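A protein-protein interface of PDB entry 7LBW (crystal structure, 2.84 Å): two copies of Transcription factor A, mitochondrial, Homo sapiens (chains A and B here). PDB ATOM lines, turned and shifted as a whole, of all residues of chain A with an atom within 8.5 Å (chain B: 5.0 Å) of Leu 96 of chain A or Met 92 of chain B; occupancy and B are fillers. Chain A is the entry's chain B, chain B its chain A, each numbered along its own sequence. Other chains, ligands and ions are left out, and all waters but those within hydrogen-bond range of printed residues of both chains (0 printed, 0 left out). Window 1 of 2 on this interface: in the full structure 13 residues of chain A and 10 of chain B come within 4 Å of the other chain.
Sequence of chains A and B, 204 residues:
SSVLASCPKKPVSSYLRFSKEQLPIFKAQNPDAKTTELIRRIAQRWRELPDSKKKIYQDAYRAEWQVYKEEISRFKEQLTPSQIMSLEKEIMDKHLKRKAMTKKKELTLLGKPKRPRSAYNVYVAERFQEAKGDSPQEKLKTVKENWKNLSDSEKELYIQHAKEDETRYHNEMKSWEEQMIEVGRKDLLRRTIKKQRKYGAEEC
The side-chain amino group (NZ) of Lys 89 of chain B is in salt-bridge range of the side-chain carboxylate (OE1) of Glu 88 of chain A (3.9 Å). The side-chain carboxylate of Glu 88 of chain B lies within salt-bridge range of the side-chain amino group of Lys 89 of chain A (3.4 Å). OD1 of Asp 93 of chain A sits close to SD of Met 92 of chain B (3.7 Å).
NZ of Lys 89 of chain B is in salt-bridge range of OD2 of Asp 93 of chain B (3.0 Å). NZ of Lys 89 of chain A lies within salt-bridge range of OD2 of Asp 93 of chain A (3.0 Å).
Lys 89 of chain B touches Met 85 of chain A (CD to CG, 3.5 Å). Met 92 of chain B touches Met 92 of chain A (CE to CG, 3.5 Å). Met 92 of chain B touches Leu 96 of chain A (SD to CD1, 3.97 Å).
Of the printed residues of chain B, Met 92 of chain A touches Met 92. Leu 96 of chain A touches just one residue of chain B: Met 92 (3.97 Å). Printed residues of chain A within 4 Å of Glu 88 of chain B: Lys 89 (3.4 Å). Of the printed residues of chain A, Lys 89 of chain B touches Met 85 and Glu 88. Of chain A, only Met 92, Asp 93 and Leu 96 come within 4 Å of Met 92 of chain B. Asp 93 of chain B touches none of the printed residues of chain A. His 95 of chain B touches none of the printed residues of chain A. The nearest residue of chain B that does not touch Leu 96 of chain A is Leu 96 of chain B (4.3 Å). The nearest printed residue of chain B that does not touch Met 92 of chain A is Leu 96 of chain B (4.1 Å).
Hydrophobic or aromatic side chains of chain A that line the printed part of chain B: Met 85, Met 92 and Leu 96. Of the 9 printed residues of chain B, 3 touch a printed residue of chain A. Printed residues of chain B that touch a printed residue of chain A: Glu 88, Lys 89 and Met 92. Hydrophobic or aromatic side chains of chain B within 4 Å of the printed part of chain A: Met 92. Along chain B the printed residues that touch a printed residue of chain A span positions 88 to 92. Among the printed residues, 6 pairs touch across the chains.
Glu 88 of chain A touches Lys 89 of chain B, and with the chains exchanged Lys 89 of chain A touches Glu 88 of chain B. Met 92 of chain B touches its own counterpart, Met 92 of chain A. Asp 93 of chain A touches Met 92 of chain B, but with the chains exchanged Met 92 of chain A does not touch Asp 93 of chain B (5.7 Å). Leu 96 of chain A touches Met 92 of chain B, but with the chains exchanged Met 92 of chain A does not touch Leu 96 of chain B (4.1 Å). Of the 6 pairs that touch across the chains among the printed residues, 3 have their exchanged pair printed and touching as well.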
ATOM      1  N   MET A  85       1.140 -14.496 -19.662  1.00  0.00           N
ATOM      2  CA  MET A  85       0.779 -13.093 -19.502  1.00  0.00           C
ATOM      3  C   MET A  85       1.239 -12.577 -18.140  1.00  0.00           C
ATOM      4  O   MET A  85       1.848 -11.509 -18.087  1.00  0.00           O
ATOM      5  CB  MET A  85      -0.722 -12.919 -19.665  1.00  0.00           C
ATOM      6  CG  MET A  85      -1.136 -11.490 -19.892  1.00  0.00           C
ATOM      7  SD  MET A  85      -2.807 -11.383 -20.614  1.00  0.00           S
ATOM      8  CE  MET A  85      -2.444 -11.807 -22.352  1.00  0.00           C
ATOM      9  N   GLU A  88       5.094 -11.922 -18.187  1.00  0.00           N
ATOM     10  CA  GLU A  88       5.347 -10.691 -18.927  1.00  0.00           C
ATOM     11  C   GLU A  88       4.929  -9.459 -18.121  1.00  0.00           C
ATOM     12  O   GLU A  88       5.645  -8.477 -18.142  1.00  0.00           O
ATOM     13  CB  GLU A  88       4.610 -10.690 -20.261  1.00  0.00           C
ATOM     14  CG  GLU A  88       5.178 -11.659 -21.264  1.00  0.00           C
ATOM     15  CD  GLU A  88       4.446 -11.722 -22.593  1.00  0.00           C
ATOM     16  OE1 GLU A  88       3.284 -11.258 -22.668  1.00  0.00           O
ATOM     17  OE2 GLU A  88       5.032 -12.268 -23.555  1.00  0.00           O
ATOM     18  N   LYS A  89       3.786  -9.488 -17.419  1.00  0.00           N
ATOM     19  CA  LYS A  89       3.375  -8.347 -16.597  1.00  0.00           C
ATOM     20  C   LYS A  89       4.353  -8.180 -15.446  1.00  0.00           C
ATOM     21  O   LYS A  89       4.756  -7.057 -15.198  1.00  0.00           O
ATOM     22  CB  LYS A  89       1.952  -8.535 -16.057  1.00  0.00           C
ATOM     23  CG  LYS A  89       1.383  -7.295 -15.392  1.00  0.00           C
ATOM     24  CD  LYS A  89       0.090  -7.594 -14.683  1.00  0.00           C
ATOM     25  CE  LYS A  89      -0.486  -6.400 -13.970  1.00  0.00           C
ATOM     26  NZ  LYS A  89       0.125  -6.170 -12.636  1.00  0.00           N
ATOM     27  N   GLU A  90       4.773  -9.279 -14.764  1.00  0.00           N
ATOM     28  CA  GLU A  90       5.726  -9.215 -13.645  1.00  0.00           C
ATOM     29  C   GLU A  90       7.054  -8.617 -14.073  1.00  0.00           C
ATOM     30  O   GLU A  90       7.618  -7.827 -13.332  1.00  0.00           O
ATOM     31  CB  GLU A  90       6.000 -10.580 -13.047  1.00  0.00           C
ATOM     32  CG  GLU A  90       4.849 -11.151 -12.259  1.00  0.00           C
ATOM     33  CD  GLU A  90       5.177 -12.517 -11.713  1.00  0.00           C
ATOM     34  OE1 GLU A  90       6.099 -12.601 -10.869  1.00  0.00           O
ATOM     35  OE2 GLU A  90       4.543 -13.504 -12.150  1.00  0.00           O
ATOM     36  N   ILE A  91       7.572  -9.008 -15.241  1.00  0.00           N
ATOM     37  CA  ILE A  91       8.830  -8.436 -15.740  1.00  0.00           C
ATOM     38  C   ILE A  91       8.686  -6.939 -15.969  1.00  0.00           C
ATOM     39  O   ILE A  91       9.521  -6.178 -15.495  1.00  0.00           O
ATOM     40  CB  ILE A  91       9.326  -9.172 -17.012  1.00  0.00           C
ATOM     41  CG1 ILE A  91       9.860 -10.582 -16.611  1.00  0.00           C
ATOM     42  CG2 ILE A  91      10.388  -8.326 -17.723  1.00  0.00           C
ATOM     43  CD1 ILE A  91      10.000 -11.574 -17.732  1.00  0.00           C
ATOM     44  N   MET A  92       7.652  -6.518 -16.684  1.00  0.00           N
ATOM     45  CA  MET A  92       7.454  -5.106 -16.923  1.00  0.00           C
ATOM     46  C   MET A  92       7.255  -4.356 -15.597  1.00  0.00           C
ATOM     47  O   MET A  92       7.965  -3.400 -15.368  1.00  0.00           O
ATOM     48  CB  MET A  92       6.297  -4.855 -17.879  1.00  0.00           C
ATOM     49  CG  MET A  92       6.281  -3.436 -18.406  1.00  0.00           C
ATOM     50  SD  MET A  92       7.892  -2.776 -19.040  1.00  0.00           S
ATOM     51  CE  MET A  92       7.940  -3.581 -20.693  1.00  0.00           C
ATOM     52  N   ASP A  93       6.389  -4.827 -14.688  1.00  0.00           N
ATOM     53  CA  ASP A  93       6.186  -4.141 -13.393  1.00  0.00           C
ATOM     54  C   ASP A  93       7.484  -3.925 -12.610  1.00  0.00           C
ATOM     55  O   ASP A  93       7.609  -2.897 -11.959  1.00  0.00           O
ATOM     56  CB  ASP A  93       5.232  -4.918 -12.477  1.00  0.00           C
ATOM     57  CG  ASP A  93       3.808  -4.970 -12.935  1.00  0.00           C
ATOM     58  OD1 ASP A  93       3.384  -4.051 -13.684  1.00  0.00           O
ATOM     59  OD2 ASP A  93       3.103  -5.912 -12.537  1.00  0.00           O
ATOM     60  N   LYS A  94       8.408  -4.905 -12.641  1.00  0.00           N
ATOM     61  CA  LYS A  94       9.693  -4.886 -11.941  1.00  0.00           C
ATOM     62  C   LYS A  94      10.542  -3.775 -12.512  1.00  0.00           C
ATOM     63  O   LYS A  94      11.082  -2.959 -11.766  1.00  0.00           O
ATOM     64  CB  LYS A  94      10.401  -6.234 -12.063  1.00  0.00           C
ATOM     65  CG  LYS A  94      11.598  -6.431 -11.136  1.00  0.00           C
ATOM     66  CD  LYS A  94      12.367  -7.710 -11.416  1.00  0.00           C
ATOM     67  CE  LYS A  94      13.681  -7.766 -10.668  1.00  0.00           C
ATOM     68  NZ  LYS A  94      14.410  -9.037 -10.912  1.00  0.00           N
ATOM     69  N   HIS A  95      10.605  -3.721 -13.839  1.00  0.00           N
ATOM     70  CA  HIS A  95      11.338  -2.702 -14.572  1.00  0.00           C
ATOM     71  C   HIS A  95      10.823  -1.296 -14.238  1.00  0.00           C
ATOM     72  O   HIS A  95      11.615  -0.404 -13.967  1.00  0.00           O
ATOM     73  CB  HIS A  95      11.230  -3.011 -16.076  1.00  0.00           C
ATOM     74  CG  HIS A  95      11.997  -2.011 -16.882  1.00  0.00           C
ATOM     75  ND1 HIS A  95      13.315  -1.689 -16.538  1.00  0.00           N
ATOM     76  CD2 HIS A  95      11.625  -1.226 -17.918  1.00  0.00           C
ATOM     77  CE1 HIS A  95      13.710  -0.768 -17.400  1.00  0.00           C
ATOM     78  NE2 HIS A  95      12.731  -0.443 -18.238  1.00  0.00           N
ATOM     79  N   LEU A  96       9.514  -1.112 -14.204  1.00  0.00           N
ATOM     80  CA  LEU A  96       8.910   0.179 -13.879  1.00  0.00           C
ATOM     81  C   LEU A  96       9.113   0.527 -12.399  1.00  0.00           C
ATOM     82  O   LEU A  96       9.321   1.693 -12.088  1.00  0.00           O
ATOM     83  CB  LEU A  96       7.420   0.190 -14.219  1.00  0.00           C
ATOM     84  CG  LEU A  96       7.051  -0.027 -15.687  1.00  0.00           C
ATOM     85  CD1 LEU A  96       5.553  -0.244 -15.834  1.00  0.00           C
ATOM     86  CD2 LEU A  96       7.501   1.112 -16.556  1.00  0.00           C
ATOM     87  N   LYS A  97       9.073  -0.461 -11.493  1.00  0.00           N
ATOM     88  CA  LYS A  97       9.296  -0.230 -10.055  1.00  0.00           C
ATOM     89  C   LYS A  97      10.714   0.284  -9.857  1.00  0.00           C
ATOM     90  O   LYS A  97      10.915   1.155  -9.041  1.00  0.00           O
ATOM     91  CB  LYS A  97       9.105  -1.510  -9.234  1.00  0.00           C
ATOM     92  CG  LYS A  97       9.064  -1.314  -7.723  1.00  0.00           C
ATOM     93  CD  LYS A  97       9.244  -2.622  -6.934  1.00  0.00           C
ATOM     94  CE  LYS A  97       9.306  -2.421  -5.435  1.00  0.00           C
ATOM     95  NZ  LYS A  97       9.553  -3.692  -4.685  1.00  0.00           N
ATOM     96  N   ARG A  98      11.689  -0.259 -10.596  1.00  0.00           N
ATOM     97  CA  ARG A  98      13.070   0.163 -10.533  1.00  0.00           C
ATOM     98  C   ARG A  98      13.213   1.560 -11.124  1.00  0.00           C
ATOM     99  O   ARG A  98      13.964   2.352 -10.569  1.00  0.00           O
ATOM    100  CB  ARG A  98      13.980  -0.828 -11.274  1.00  0.00           C
ATOM    101  CG  ARG A  98      15.485  -0.511 -11.126  1.00  0.00           C
ATOM    102  CD  ARG A  98      16.410  -1.611 -11.627  1.00  0.00           C
ATOM    103  NE  ARG A  98      16.287  -2.849 -10.853  1.00  0.00           N
ATOM    104  CZ  ARG A  98      16.993  -3.955 -11.071  1.00  0.00           C
ATOM    105  NH1 ARG A  98      17.891  -4.000 -12.049  1.00  0.00           N
ATOM    106  NH2 ARG A  98      16.802  -5.030 -10.314  1.00  0.00           N
ATOM    107  N   LYS A  99      12.519   1.870 -12.233  1.00  0.00           N
ATOM    108  CA  LYS A  99      12.579   3.211 -12.832  1.00  0.00           C
ATOM    109  C   LYS A  99      12.025   4.246 -11.849  1.00  0.00           C
ATOM    110  O   LYS A  99      12.708   5.204 -11.504  1.00  0.00           O
ATOM    111  CB  LYS A  99      11.834   3.281 -14.181  1.00  0.00           C
ATOM    112  CG  LYS A  99      12.753   2.996 -15.353  1.00  0.00           C
ATOM    113  CD  LYS A  99      12.088   3.042 -16.720  1.00  0.00           C
ATOM    114  CE  LYS A  99      11.458   4.364 -17.043  1.00  0.00           C
ATOM    115  NZ  LYS A  99      11.407   4.596 -18.512  1.00  0.00           N
ATOM    116  N   ALA A 100      10.827   4.008 -11.348  1.00  0.00           N
ATOM    117  CA  ALA A 100      10.161   4.904 -10.403  1.00  0.00           C
ATOM    118  C   ALA A 100      11.000   5.150  -9.143  1.00  0.00           C
ATOM    119  O   ALA A 100      11.101   6.278  -8.675  1.00  0.00           O
ATOM    120  CB  ALA A 100       8.826   4.319 -10.011  1.00  0.00           C
ATOM    121  N   MET A 101      11.586   4.094  -8.600  1.00  0.00           N
ATOM    122  CA  MET A 101      12.402   4.142  -7.385  1.00  0.00           C
ATOM    123  C   MET A 101      13.680   4.933  -7.632  1.00  0.00           C
ATOM    124  O   MET A 101      14.062   5.719  -6.786  1.00  0.00           O
ATOM    125  CB  MET A 101      12.716   2.720  -6.922  1.00  0.00           C
ATOM    126  CG  MET A 101      13.485   2.641  -5.664  1.00  0.00           C
ATOM    127  SD  MET A 101      13.246   1.061  -4.820  1.00  0.00           S
ATOM    128  CE  MET A 101      14.533   1.166  -3.518  1.00  0.00           C
ATOM    129  N   THR A 102      14.319   4.751  -8.795  1.00  0.00           N
ATOM    130  CA  THR A 102      15.529   5.479  -9.173  1.00  0.00           C
ATOM    131  C   THR A 102      15.221   6.979  -9.276  1.00  0.00           C
ATOM    132  O   THR A 102      16.028   7.786  -8.811  1.00  0.00           O
ATOM    133  CB  THR A 102      16.121   4.891 -10.483  1.00  0.00           C
ATOM    134  OG1 THR A 102      16.742   3.641 -10.198  1.00  0.00           O
ATOM    135  CG2 THR A 102      17.143   5.794 -11.130  1.00  0.00           C
ATOM    136  N   LYS A 103      14.072   7.347  -9.888  1.00  0.00           N
ATOM    137  CA  LYS A 103      13.648   8.739 -10.011  1.00  0.00           C
ATOM    138  C   LYS A 103      13.392   9.368  -8.641  1.00  0.00           C
ATOM    139  O   LYS A 103      13.801  10.496  -8.432  1.00  0.00           O
ATOM    140  CB  LYS A 103      12.396   8.871 -10.892  1.00  0.00           C
ATOM    141  CG  LYS A 103      12.654   8.552 -12.363  1.00  0.00           C
ATOM    142  CD  LYS A 103      11.362   8.661 -13.202  1.00  0.00           C
ATOM    143  CE  LYS A 103      11.333   7.831 -14.477  1.00  0.00           C
ATOM    144  NZ  LYS A 103      10.163   6.899 -14.509  1.00  0.00           N
ATOM    145  N   GLU B  88      -5.209  -4.837 -16.195  1.00  0.00           N
ATOM    146  CA  GLU B  88      -4.078  -4.018 -15.767  1.00  0.00           C
ATOM    147  C   GLU B  88      -2.942  -4.061 -16.764  1.00  0.00           C
ATOM    148  O   GLU B  88      -2.345  -3.026 -16.997  1.00  0.00           O
ATOM    149  CB  GLU B  88      -3.548  -4.445 -14.405  1.00  0.00           C
ATOM    150  CG  GLU B  88      -4.498  -4.127 -13.260  1.00  0.00           C
ATOM    151  CD  GLU B  88      -4.030  -4.589 -11.892  1.00  0.00           C
ATOM    152  OE1 GLU B  88      -3.115  -5.444 -11.817  1.00  0.00           O
ATOM    153  OE2 GLU B  88      -4.604  -4.105 -10.890  1.00  0.00           O
ATOM    154  N   LYS B  89      -2.619  -5.218 -17.352  1.00  0.00           N
ATOM    155  CA  LYS B  89      -1.559  -5.290 -18.370  1.00  0.00           C
ATOM    156  C   LYS B  89      -1.990  -4.521 -19.607  1.00  0.00           C
ATOM    157  O   LYS B  89      -1.192  -3.762 -20.109  1.00  0.00           O
ATOM    158  CB  LYS B  89      -1.232  -6.740 -18.744  1.00  0.00           C
ATOM    159  CG  LYS B  89       0.003  -6.883 -19.612  1.00  0.00           C
ATOM    160  CD  LYS B  89       0.151  -8.288 -20.139  1.00  0.00           C
ATOM    161  CE  LYS B  89       1.356  -8.453 -21.040  1.00  0.00           C
ATOM    162  NZ  LYS B  89       1.120  -7.984 -22.431  1.00  0.00           N
ATOM    163  N   GLU B  90      -3.254  -4.668 -20.074  1.00  0.00           N
ATOM    164  CA  GLU B  90      -3.759  -3.941 -21.252  1.00  0.00           C
ATOM    165  C   GLU B  90      -3.694  -2.440 -21.059  1.00  0.00           C
ATOM    166  O   GLU B  90      -3.298  -1.736 -21.981  1.00  0.00           O
ATOM    167  CB  GLU B  90      -5.212  -4.318 -21.552  1.00  0.00           C
ATOM    168  CG  GLU B  90      -5.383  -5.716 -22.100  1.00  0.00           C
ATOM    169  CD  GLU B  90      -6.838  -6.053 -22.344  1.00  0.00           C
ATOM    170  OE1 GLU B  90      -7.436  -5.380 -23.217  1.00  0.00           O
ATOM    171  OE2 GLU B  90      -7.388  -6.944 -21.644  1.00  0.00           O
ATOM    172  N   ILE B  91      -4.093  -1.943 -19.869  1.00  0.00           N
ATOM    173  CA  ILE B  91      -4.033  -0.514 -19.585  1.00  0.00           C
ATOM    174  C   ILE B  91      -2.577  -0.055 -19.620  1.00  0.00           C
ATOM    175  O   ILE B  91      -2.300   0.922 -20.275  1.00  0.00           O
ATOM    176  CB  ILE B  91      -4.718  -0.151 -18.248  1.00  0.00           C
ATOM    177  CG1 ILE B  91      -6.253  -0.271 -18.398  1.00  0.00           C
ATOM    178  CG2 ILE B  91      -4.304   1.259 -17.774  1.00  0.00           C
ATOM    179  CD1 ILE B  91      -7.038  -0.343 -17.105  1.00  0.00           C
ATOM    180  N   MET B  92      -1.659  -0.778 -18.937  1.00  0.00           N
ATOM    181  CA  MET B  92      -0.207  -0.499 -18.885  1.00  0.00           C
ATOM    182  C   MET B  92       0.394  -0.480 -20.281  1.00  0.00           C
ATOM    183  O   MET B  92       1.094   0.462 -20.614  1.00  0.00           O
ATOM    184  CB  MET B  92       0.507  -1.564 -18.024  1.00  0.00           C
ATOM    185  CG  MET B  92       2.005  -1.352 -17.831  1.00  0.00           C
ATOM    186  SD  MET B  92       2.833  -2.837 -17.129  1.00  0.00           S
ATOM    187  CE  MET B  92       2.855  -4.026 -18.637  1.00  0.00           C
ATOM    188  N   ASP B  93       0.114  -1.492 -21.107  1.00  0.00           N
ATOM    189  CA  ASP B  93       0.651  -1.542 -22.485  1.00  0.00           C
ATOM    190  C   ASP B  93       0.248  -0.345 -23.362  1.00  0.00           C
ATOM    191  O   ASP B  93       1.056   0.137 -24.161  1.00  0.00           O
ATOM    192  CB  ASP B  93       0.193  -2.830 -23.184  1.00  0.00           C
ATOM    193  CG  ASP B  93       0.785  -4.104 -22.628  1.00  0.00           C
ATOM    194  OD1 ASP B  93       1.895  -4.040 -22.036  1.00  0.00           O
ATOM    195  OD2 ASP B  93       0.147  -5.174 -22.792  1.00  0.00           O
ATOM    196  N   LYS B  94      -1.020   0.088 -23.225  1.00  0.00           N
ATOM    197  CA  LYS B  94      -1.604   1.187 -23.998  1.00  0.00           C
ATOM    198  C   LYS B  94      -0.907   2.484 -23.606  1.00  0.00           C
ATOM    199  O   LYS B  94      -0.477   3.246 -24.464  1.00  0.00           O
ATOM    200  CB  LYS B  94      -3.133   1.257 -23.702  1.00  0.00           C
ATOM    201  CG  LYS B  94      -3.919   2.132 -24.652  1.00  0.00           C
ATOM    202  CD  LYS B  94      -5.391   2.297 -24.225  1.00  0.00           C
ATOM    203  CE  LYS B  94      -6.076   3.369 -25.049  1.00  0.00           C
ATOM    204  NZ  LYS B  94      -7.504   3.536 -24.672  1.00  0.00           N
ATOM    205  N   HIS B  95      -0.751   2.695 -22.310  1.00  0.00           N
ATOM    206  CA  HIS B  95      -0.070   3.849 -21.736  1.00  0.00           C
ATOM    207  C   HIS B  95       1.377   3.929 -22.205  1.00  0.00           C
ATOM    208  O   HIS B  95       1.819   4.998 -22.598  1.00  0.00           O
ATOM    209  CB  HIS B  95      -0.144   3.774 -20.211  1.00  0.00           C
ATOM    210  CG  HIS B  95       0.588   4.777 -19.387  1.00  0.00           C
ATOM    211  ND1 HIS B  95       0.999   4.415 -18.112  1.00  0.00           N
ATOM    212  CD2 HIS B  95       1.036   6.037 -19.643  1.00  0.00           C
ATOM    213  CE1 HIS B  95       1.673   5.440 -17.625  1.00  0.00           C
ATOM    214  NE2 HIS B  95       1.745   6.439 -18.507  1.00  0.00           N
ATOM    215  N   LEU B  96       2.100   2.806 -22.209  1.00  0.00           N
ATOM    216  CA  LEU B  96       3.484   2.766 -22.666  1.00  0.00           C
ATOM    217  C   LEU B  96       3.574   3.006 -24.160  1.00  0.00           C
ATOM    218  O   LEU B  96       4.501   3.687 -24.584  1.00  0.00           O
ATOM    219  CB  LEU B  96       4.150   1.436 -22.300  1.00  0.00           C
ATOM    220  CG  LEU B  96       4.263   1.127 -20.803  1.00  0.00           C
ATOM    221  CD1 LEU B  96       4.718  -0.303 -20.600  1.00  0.00           C
ATOM    222  CD2 LEU B  96       5.185   2.076 -20.081  1.00  0.00           C
